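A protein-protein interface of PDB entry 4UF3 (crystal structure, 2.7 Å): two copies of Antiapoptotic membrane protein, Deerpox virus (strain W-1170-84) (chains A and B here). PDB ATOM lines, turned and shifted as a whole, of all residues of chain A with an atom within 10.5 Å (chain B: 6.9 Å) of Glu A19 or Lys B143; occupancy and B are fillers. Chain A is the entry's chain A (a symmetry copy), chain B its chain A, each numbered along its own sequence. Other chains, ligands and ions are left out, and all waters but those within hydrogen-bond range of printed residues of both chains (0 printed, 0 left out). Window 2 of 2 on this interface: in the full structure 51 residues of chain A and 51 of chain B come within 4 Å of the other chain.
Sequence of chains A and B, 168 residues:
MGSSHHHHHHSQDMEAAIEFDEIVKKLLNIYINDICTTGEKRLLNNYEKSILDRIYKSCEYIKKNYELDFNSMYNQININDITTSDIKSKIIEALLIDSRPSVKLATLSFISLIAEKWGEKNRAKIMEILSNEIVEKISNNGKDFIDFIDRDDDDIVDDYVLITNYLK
Of the printed residues of chain B, Ala A17 touches Asn B141 (3.8 Å) and Lys B143 (3.7 Å).
Printed residues of chain B within 4 Å of Phe A20: Lys B143 and Ile B146.
Of the printed residues of chain B, Ile A23 touches Ile B146.
Of the printed residues of chain A, Ser B139 touches Asp A21, Val A24 and Lys A25.
Printed residues of chain A within 4 Å of Asn B141: Ala A17 (3.8 Å) and Asp A21 (3.9 Å).
Lys B143 touches three residues of chain A.
Phe B145 touches none of the printed residues of chain A.
Of chain A, only Phe A20, Ile A23 and Val A24 come within 4 Å of Ile B146.
No residue of chain A comes within 4 Å of Asp B147.
Ile B149 touches none of the printed residues of chain A.
The nearest residue of chain B that does not touch Glu A19 is Gly B142 (6.7 Å).
The nearest residue of chain A that does not touch Lys B143 is Asp A21 (4.6 Å).
The nearest printed residue of chain A that does not touch Ser B139 is Phe A20 (5.2 Å).
O of Ala A17 touches OD1 of Asn B141, 3.8 Å away.
Ala A17 touches Lys B143 (CB to CD, 3.7 Å).
Phe A20 touches Lys B143 (CB to N, 3.7 Å).
CD1 of Ile B146 touches CD1 of Phe A20, at 3.5 Å.
OD2 of Asp A21 touches N of Asn B141, 3.9 Å away.
CG2 of Ile A23 touches CD1 of Ile B146, at 3.8 Å.
Val A24 touches Ser B139.
Gly B142 touches Val A24.
Val A24 touches Ile B146.
The side-chain amino group (NZ) of Lys B143 lies within salt-bridge range of the side-chain carboxylate (OE2) of Glu A19 (3.1 Å).
N of Lys A25 lies close to OG of Ser B139.
The backbone carbonyl oxygen (O) of Ser B139 lies close to the side-chain carboxylate (OD1) of Asp A21, at 3.4 Å.
The side-chain carboxylate (OD1) of Asp A21 sits at hydrogen-bond distance from the backbone NH (N) of Gly B142.
No position is printed for both chains.
Of the 13 pairs that touch across the chains among the printed residues, none has its exchanged pair printed and touching as well.
Of the 11 printed residues of chain B, 5 touch a printed residue of chain A.
Printed residues of chain B that touch a printed residue of chain A: Ser B139, Asn B141, Gly B142, Lys B143 and Ile B146.
Hydrophobic or aromatic side chains of chain B that line the printed part of chain A: Ile B146.
Hydrophobic or aromatic side chains of chain A that line the printed part of chain B: Ala A17, Phe A20, Ile A23 and Val A24.
Among the printed residues, 13 pairs touch across the chains.
ND2 of Asn B141 is in hydrogen-bond range of OD2 of Asp B144 (3.1 Å).
OE2 of Glu A22 is in salt-bridge range of NZ of Lys A25 (2.7 Å).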
ATOM      1  N   ALA A  16     -23.602  -6.797  16.201  1.00  0.00           N
ATOM      2  CA  ALA A  16     -23.821  -8.029  15.452  1.00  0.00           C
ATOM      3  C   ALA A  16     -23.560  -7.827  13.963  1.00  0.00           C
ATOM      4  O   ALA A  16     -23.250  -6.722  13.519  1.00  0.00           O
ATOM      5  CB  ALA A  16     -25.237  -8.540  15.674  1.00  0.00           C
ATOM      6  N   ALA A  17     -23.677  -8.908  13.200  1.00  0.00           N
ATOM      7  CA  ALA A  17     -23.506  -8.843  11.753  1.00  0.00           C
ATOM      8  C   ALA A  17     -24.837  -8.537  11.080  1.00  0.00           C
ATOM      9  O   ALA A  17     -25.674  -9.422  10.910  1.00  0.00           O
ATOM     10  CB  ALA A  17     -22.928 -10.139  11.225  1.00  0.00           C
ATOM     11  N   ILE A  18     -25.026  -7.277  10.703  1.00  0.00           N
ATOM     12  CA  ILE A  18     -26.295  -6.824  10.145  1.00  0.00           C
ATOM     13  C   ILE A  18     -26.178  -6.404   8.682  1.00  0.00           C
ATOM     14  O   ILE A  18     -27.179  -6.063   8.047  1.00  0.00           O
ATOM     15  CB  ILE A  18     -26.857  -5.638  10.942  1.00  0.00           C
ATOM     16  CG1 ILE A  18     -25.942  -4.419  10.789  1.00  0.00           C
ATOM     17  CG2 ILE A  18     -27.015  -6.014  12.410  1.00  0.00           C
ATOM     18  CD1 ILE A  18     -26.481  -3.157  11.427  1.00  0.00           C
ATOM     19  N   GLU A  19     -24.964  -6.449   8.141  1.00  0.00           N
ATOM     20  CA  GLU A  19     -24.686  -5.840   6.842  1.00  0.00           C
ATOM     21  C   GLU A  19     -25.310  -6.581   5.656  1.00  0.00           C
ATOM     22  O   GLU A  19     -25.099  -6.203   4.501  1.00  0.00           O
ATOM     23  CB  GLU A  19     -23.174  -5.721   6.628  1.00  0.00           C
ATOM     24  CG  GLU A  19     -22.452  -7.042   6.424  1.00  0.00           C
ATOM     25  CD  GLU A  19     -22.065  -7.718   7.727  1.00  0.00           C
ATOM     26  OE1 GLU A  19     -22.625  -7.354   8.785  1.00  0.00           O
ATOM     27  OE2 GLU A  19     -21.189  -8.609   7.691  1.00  0.00           O
ATOM     28  N   PHE A  20     -26.078  -7.627   5.934  1.00  0.00           N
ATOM     29  CA  PHE A  20     -26.748  -8.384   4.882  1.00  0.00           C
ATOM     30  C   PHE A  20     -28.263  -8.398   5.075  1.00  0.00           C
ATOM     31  O   PHE A  20     -28.982  -9.079   4.344  1.00  0.00           O
ATOM     32  CB  PHE A  20     -26.219  -9.819   4.836  1.00  0.00           C
ATOM     33  CG  PHE A  20     -24.950  -9.977   4.053  1.00  0.00           C
ATOM     34  CD1 PHE A  20     -24.983 -10.082   2.673  1.00  0.00           C
ATOM     35  CD2 PHE A  20     -23.723 -10.030   4.696  1.00  0.00           C
ATOM     36  CE1 PHE A  20     -23.819 -10.232   1.946  1.00  0.00           C
ATOM     37  CE2 PHE A  20     -22.553 -10.178   3.975  1.00  0.00           C
ATOM     38  CZ  PHE A  20     -22.601 -10.276   2.596  1.00  0.00           C
ATOM     39  N   ASP A  21     -28.743  -7.646   6.059  1.00  0.00           N
ATOM     40  CA  ASP A  21     -30.164  -7.637   6.394  1.00  0.00           C
ATOM     41  C   ASP A  21     -31.020  -7.033   5.283  1.00  0.00           C
ATOM     42  O   ASP A  21     -32.121  -7.514   5.016  1.00  0.00           O
ATOM     43  CB  ASP A  21     -30.398  -6.878   7.703  1.00  0.00           C
ATOM     44  CG  ASP A  21     -29.764  -7.563   8.897  1.00  0.00           C
ATOM     45  OD1 ASP A  21     -28.827  -8.363   8.699  1.00  0.00           O
ATOM     46  OD2 ASP A  21     -30.201  -7.298  10.036  1.00  0.00           O
ATOM     47  N   GLU A  22     -30.515  -5.986   4.636  1.00  0.00           N
ATOM     48  CA  GLU A  22     -31.267  -5.309   3.587  1.00  0.00           C
ATOM     49  C   GLU A  22     -31.273  -6.115   2.290  1.00  0.00           C
ATOM     50  O   GLU A  22     -32.229  -6.056   1.517  1.00  0.00           O
ATOM     51  CB  GLU A  22     -30.701  -3.909   3.337  1.00  0.00           C
ATOM     52  CG  GLU A  22     -31.061  -2.898   4.416  1.00  0.00           C
ATOM     53  CD  GLU A  22     -32.554  -2.830   4.666  1.00  0.00           C
ATOM     54  OE1 GLU A  22     -33.314  -2.675   3.685  1.00  0.00           O
ATOM     55  OE2 GLU A  22     -32.972  -2.946   5.840  1.00  0.00           O
ATOM     56  N   ILE A  23     -30.202  -6.868   2.061  1.00  0.00           N
ATOM     57  CA  ILE A  23     -30.113  -7.747   0.899  1.00  0.00           C
ATOM     58  C   ILE A  23     -31.183  -8.838   0.975  1.00  0.00           C
ATOM     59  O   ILE A  23     -31.863  -9.118  -0.014  1.00  0.00           O
ATOM     60  CB  ILE A  23     -28.709  -8.380   0.783  1.00  0.00           C
ATOM     61  CG1 ILE A  23     -27.739  -7.388   0.143  1.00  0.00           C
ATOM     62  CG2 ILE A  23     -28.751  -9.670  -0.026  1.00  0.00           C
ATOM     63  CD1 ILE A  23     -26.288  -7.797   0.246  1.00  0.00           C
ATOM     64  N   VAL A  24     -31.351  -9.418   2.160  1.00  0.00           N
ATOM     65  CA  VAL A  24     -32.353 -10.460   2.366  1.00  0.00           C
ATOM     66  C   VAL A  24     -33.763  -9.903   2.195  1.00  0.00           C
ATOM     67  O   VAL A  24     -34.615 -10.543   1.585  1.00  0.00           O
ATOM     68  CB  VAL A  24     -32.219 -11.110   3.760  1.00  0.00           C
ATOM     69  CG1 VAL A  24     -33.298 -12.166   3.970  1.00  0.00           C
ATOM     70  CG2 VAL A  24     -30.847 -11.726   3.911  1.00  0.00           C
ATOM     71  N   LYS A  25     -34.003  -8.707   2.728  1.00  0.00           N
ATOM     72  CA  LYS A  25     -35.297  -8.046   2.568  1.00  0.00           C
ATOM     73  C   LYS A  25     -35.669  -7.877   1.105  1.00  0.00           C
ATOM     74  O   LYS A  25     -36.761  -8.249   0.677  1.00  0.00           O
ATOM     75  CB  LYS A  25     -35.296  -6.672   3.237  1.00  0.00           C
ATOM     76  CG  LYS A  25     -35.667  -6.684   4.694  1.00  0.00           C
ATOM     77  CD  LYS A  25     -35.688  -5.282   5.265  1.00  0.00           C
ATOM     78  CE  LYS A  25     -35.223  -5.284   6.711  1.00  0.00           C
ATOM     79  NZ  LYS A  25     -35.064  -3.901   7.233  1.00  0.00           N
ATOM     80  N   SER B 139     -35.073 -11.459   7.924  1.00  0.00           N
ATOM     81  CA  SER B 139     -33.910 -10.651   7.575  1.00  0.00           C
ATOM     82  C   SER B 139     -32.989 -10.406   8.769  1.00  0.00           C
ATOM     83  O   SER B 139     -31.819 -10.065   8.588  1.00  0.00           O
ATOM     84  CB  SER B 139     -34.355  -9.321   6.967  1.00  0.00           C
ATOM     85  OG  SER B 139     -35.004  -9.540   5.728  1.00  0.00           O
ATOM     86  N   ASN B 140     -33.521 -10.564   9.980  1.00  0.00           N
ATOM     87  CA  ASN B 140     -32.706 -10.500  11.189  1.00  0.00           C
ATOM     88  C   ASN B 140     -31.555 -11.489  11.098  1.00  0.00           C
ATOM     89  O   ASN B 140     -31.775 -12.669  10.821  1.00  0.00           O
ATOM     90  CB  ASN B 140     -33.547 -10.782  12.436  1.00  0.00           C
ATOM     91  CG  ASN B 140     -34.315  -9.562  12.913  1.00  0.00           C
ATOM     92  OD1 ASN B 140     -35.484  -9.655  13.292  1.00  0.00           O
ATOM     93  ND2 ASN B 140     -33.658  -8.409  12.897  1.00  0.00           N
ATOM     94  N   ASN B 141     -30.335 -11.002  11.322  1.00  0.00           N
ATOM     95  CA  ASN B 141     -29.127 -11.801  11.129  1.00  0.00           C
ATOM     96  C   ASN B 141     -29.137 -12.432   9.740  1.00  0.00           C
ATOM     97  O   ASN B 141     -29.074 -13.653   9.596  1.00  0.00           O
ATOM     98  CB  ASN B 141     -29.009 -12.874  12.216  1.00  0.00           C
ATOM     99  CG  ASN B 141     -27.640 -13.527  12.253  1.00  0.00           C
ATOM    100  OD1 ASN B 141     -26.699 -13.065  11.608  1.00  0.00           O
ATOM    101  ND2 ASN B 141     -27.524 -14.609  13.016  1.00  0.00           N
ATOM    102  N   GLY B 142     -29.245 -11.584   8.722  1.00  0.00           N
ATOM    103  CA  GLY B 142     -29.349 -12.038   7.348  1.00  0.00           C
ATOM    104  C   GLY B 142     -28.099 -12.747   6.875  1.00  0.00           C
ATOM    105  O   GLY B 142     -28.163 -13.653   6.045  1.00  0.00           O
ATOM    106  N   LYS B 143     -26.959 -12.330   7.416  1.00  0.00           N
ATOM    107  CA  LYS B 143     -25.674 -12.920   7.068  1.00  0.00           C
ATOM    108  C   LYS B 143     -25.647 -14.416   7.359  1.00  0.00           C
ATOM    109  O   LYS B 143     -25.182 -15.207   6.537  1.00  0.00           O
ATOM    110  CB  LYS B 143     -24.543 -12.220   7.822  1.00  0.00           C
ATOM    111  CG  LYS B 143     -23.167 -12.781   7.517  1.00  0.00           C
ATOM    112  CD  LYS B 143     -22.065 -11.944   8.135  1.00  0.00           C
ATOM    113  CE  LYS B 143     -20.735 -12.230   7.467  1.00  0.00           C
ATOM    114  NZ  LYS B 143     -19.678 -11.278   7.901  1.00  0.00           N
ATOM    115  N   ASP B 144     -26.146 -14.798   8.531  1.00  0.00           N
ATOM    116  CA  ASP B 144     -26.235 -16.205   8.898  1.00  0.00           C
ATOM    117  C   ASP B 144     -27.218 -16.949   7.998  1.00  0.00           C
ATOM    118  O   ASP B 144     -27.023 -18.126   7.699  1.00  0.00           O
ATOM    119  CB  ASP B 144     -26.643 -16.355  10.366  1.00  0.00           C
ATOM    120  CG  ASP B 144     -25.460 -16.259  11.314  1.00  0.00           C
ATOM    121  OD1 ASP B 144     -24.477 -15.561  10.982  1.00  0.00           O
ATOM    122  OD2 ASP B 144     -25.517 -16.886  12.395  1.00  0.00           O
ATOM    123  N   PHE B 145     -28.271 -16.259   7.567  1.00  0.00           N
ATOM    124  CA  PHE B 145     -29.251 -16.852   6.665  1.00  0.00           C
ATOM    125  C   PHE B 145     -28.647 -17.090   5.290  1.00  0.00           C
ATOM    126  O   PHE B 145     -28.858 -18.138   4.683  1.00  0.00           O
ATOM    127  CB  PHE B 145     -30.493 -15.963   6.538  1.00  0.00           C
ATOM    128  CG  PHE B 145     -31.511 -16.486   5.563  1.00  0.00           C
ATOM    129  CD1 PHE B 145     -32.338 -17.540   5.909  1.00  0.00           C
ATOM    130  CD2 PHE B 145     -31.637 -15.930   4.304  1.00  0.00           C
ATOM    131  CE1 PHE B 145     -33.270 -18.029   5.017  1.00  0.00           C
ATOM    132  CE2 PHE B 145     -32.569 -16.411   3.407  1.00  0.00           C
ATOM    133  CZ  PHE B 145     -33.385 -17.466   3.763  1.00  0.00           C
ATOM    134  N   ILE B 146     -27.904 -16.104   4.800  1.00  0.00           N
ATOM    135  CA  ILE B 146     -27.291 -16.194   3.481  1.00  0.00           C
ATOM    136  C   ILE B 146     -26.222 -17.283   3.456  1.00  0.00           C
ATOM    137  O   ILE B 146     -26.122 -18.038   2.491  1.00  0.00           O
ATOM    138  CB  ILE B 146     -26.683 -14.837   3.050  1.00  0.00           C
ATOM    139  CG1 ILE B 146     -27.800 -13.829   2.762  1.00  0.00           C
ATOM    140  CG2 ILE B 146     -25.799 -15.001   1.823  1.00  0.00           C
ATOM    141  CD1 ILE B 146     -27.345 -12.591   2.023  1.00  0.00           C
ATOM    142  N   ASP B 147     -25.445 -17.378   4.530  1.00  0.00           N
ATOM    143  CA  ASP B 147     -24.387 -18.377   4.621  1.00  0.00           C
ATOM    144  C   ASP B 147     -24.933 -19.798   4.740  1.00  0.00           C
ATOM    145  O   ASP B 147     -24.315 -20.747   4.257  1.00  0.00           O
ATOM    146  CB  ASP B 147     -23.466 -18.074   5.806  1.00  0.00           C
ATOM    147  CG  ASP B 147     -22.644 -16.813   5.601  1.00  0.00           C
ATOM    148  OD1 ASP B 147     -22.544 -16.343   4.443  1.00  0.00           O
ATOM    149  OD2 ASP B 147     -22.093 -16.300   6.601  1.00  0.00           O
ATOM    150  N   PHE B 148     -26.080 -19.943   5.395  1.00  0.00           N
ATOM    151  CA  PHE B 148     -26.737 -21.240   5.494  1.00  0.00           C
ATOM    152  C   PHE B 148     -27.214 -21.689   4.123  1.00  0.00           C
ATOM    153  O   PHE B 148     -27.193 -22.877   3.798  1.00  0.00           O
ATOM    154  CB  PHE B 148     -27.918 -21.178   6.467  1.00  0.00           C
ATOM    155  CG  PHE B 148     -28.768 -22.421   6.472  1.00  0.00           C
ATOM    156  CD1 PHE B 148     -28.409 -23.515   7.243  1.00  0.00           C
ATOM    157  CD2 PHE B 148     -29.930 -22.493   5.715  1.00  0.00           C
ATOM    158  CE1 PHE B 148     -29.185 -24.658   7.253  1.00  0.00           C
ATOM    159  CE2 PHE B 148     -30.708 -23.637   5.720  1.00  0.00           C
ATOM    160  CZ  PHE B 148     -30.335 -24.718   6.491  1.00  0.00           C
ATOM    161  N   ILE B 149     -27.648 -20.718   3.328  1.00  0.00           N
ATOM    162  CA  ILE B 149     -28.220 -20.976   2.018  1.00  0.00           C
ATOM    163  C   ILE B 149     -27.137 -21.211   0.968  1.00  0.00           C
ATOM    164  O   ILE B 149     -27.278 -22.068   0.094  1.00  0.00           O
ATOM    165  CB  ILE B 149     -29.132 -19.804   1.589  1.00  0.00           C
ATOM    166  CG1 ILE B 149     -30.450 -19.858   2.353  1.00  0.00           C
ATOM    167  CG2 ILE B 149     -29.433 -19.858   0.115  1.00  0.00           C
ATOM    168  CD1 ILE B 149     -31.295 -21.060   1.995  1.00  0.00           C
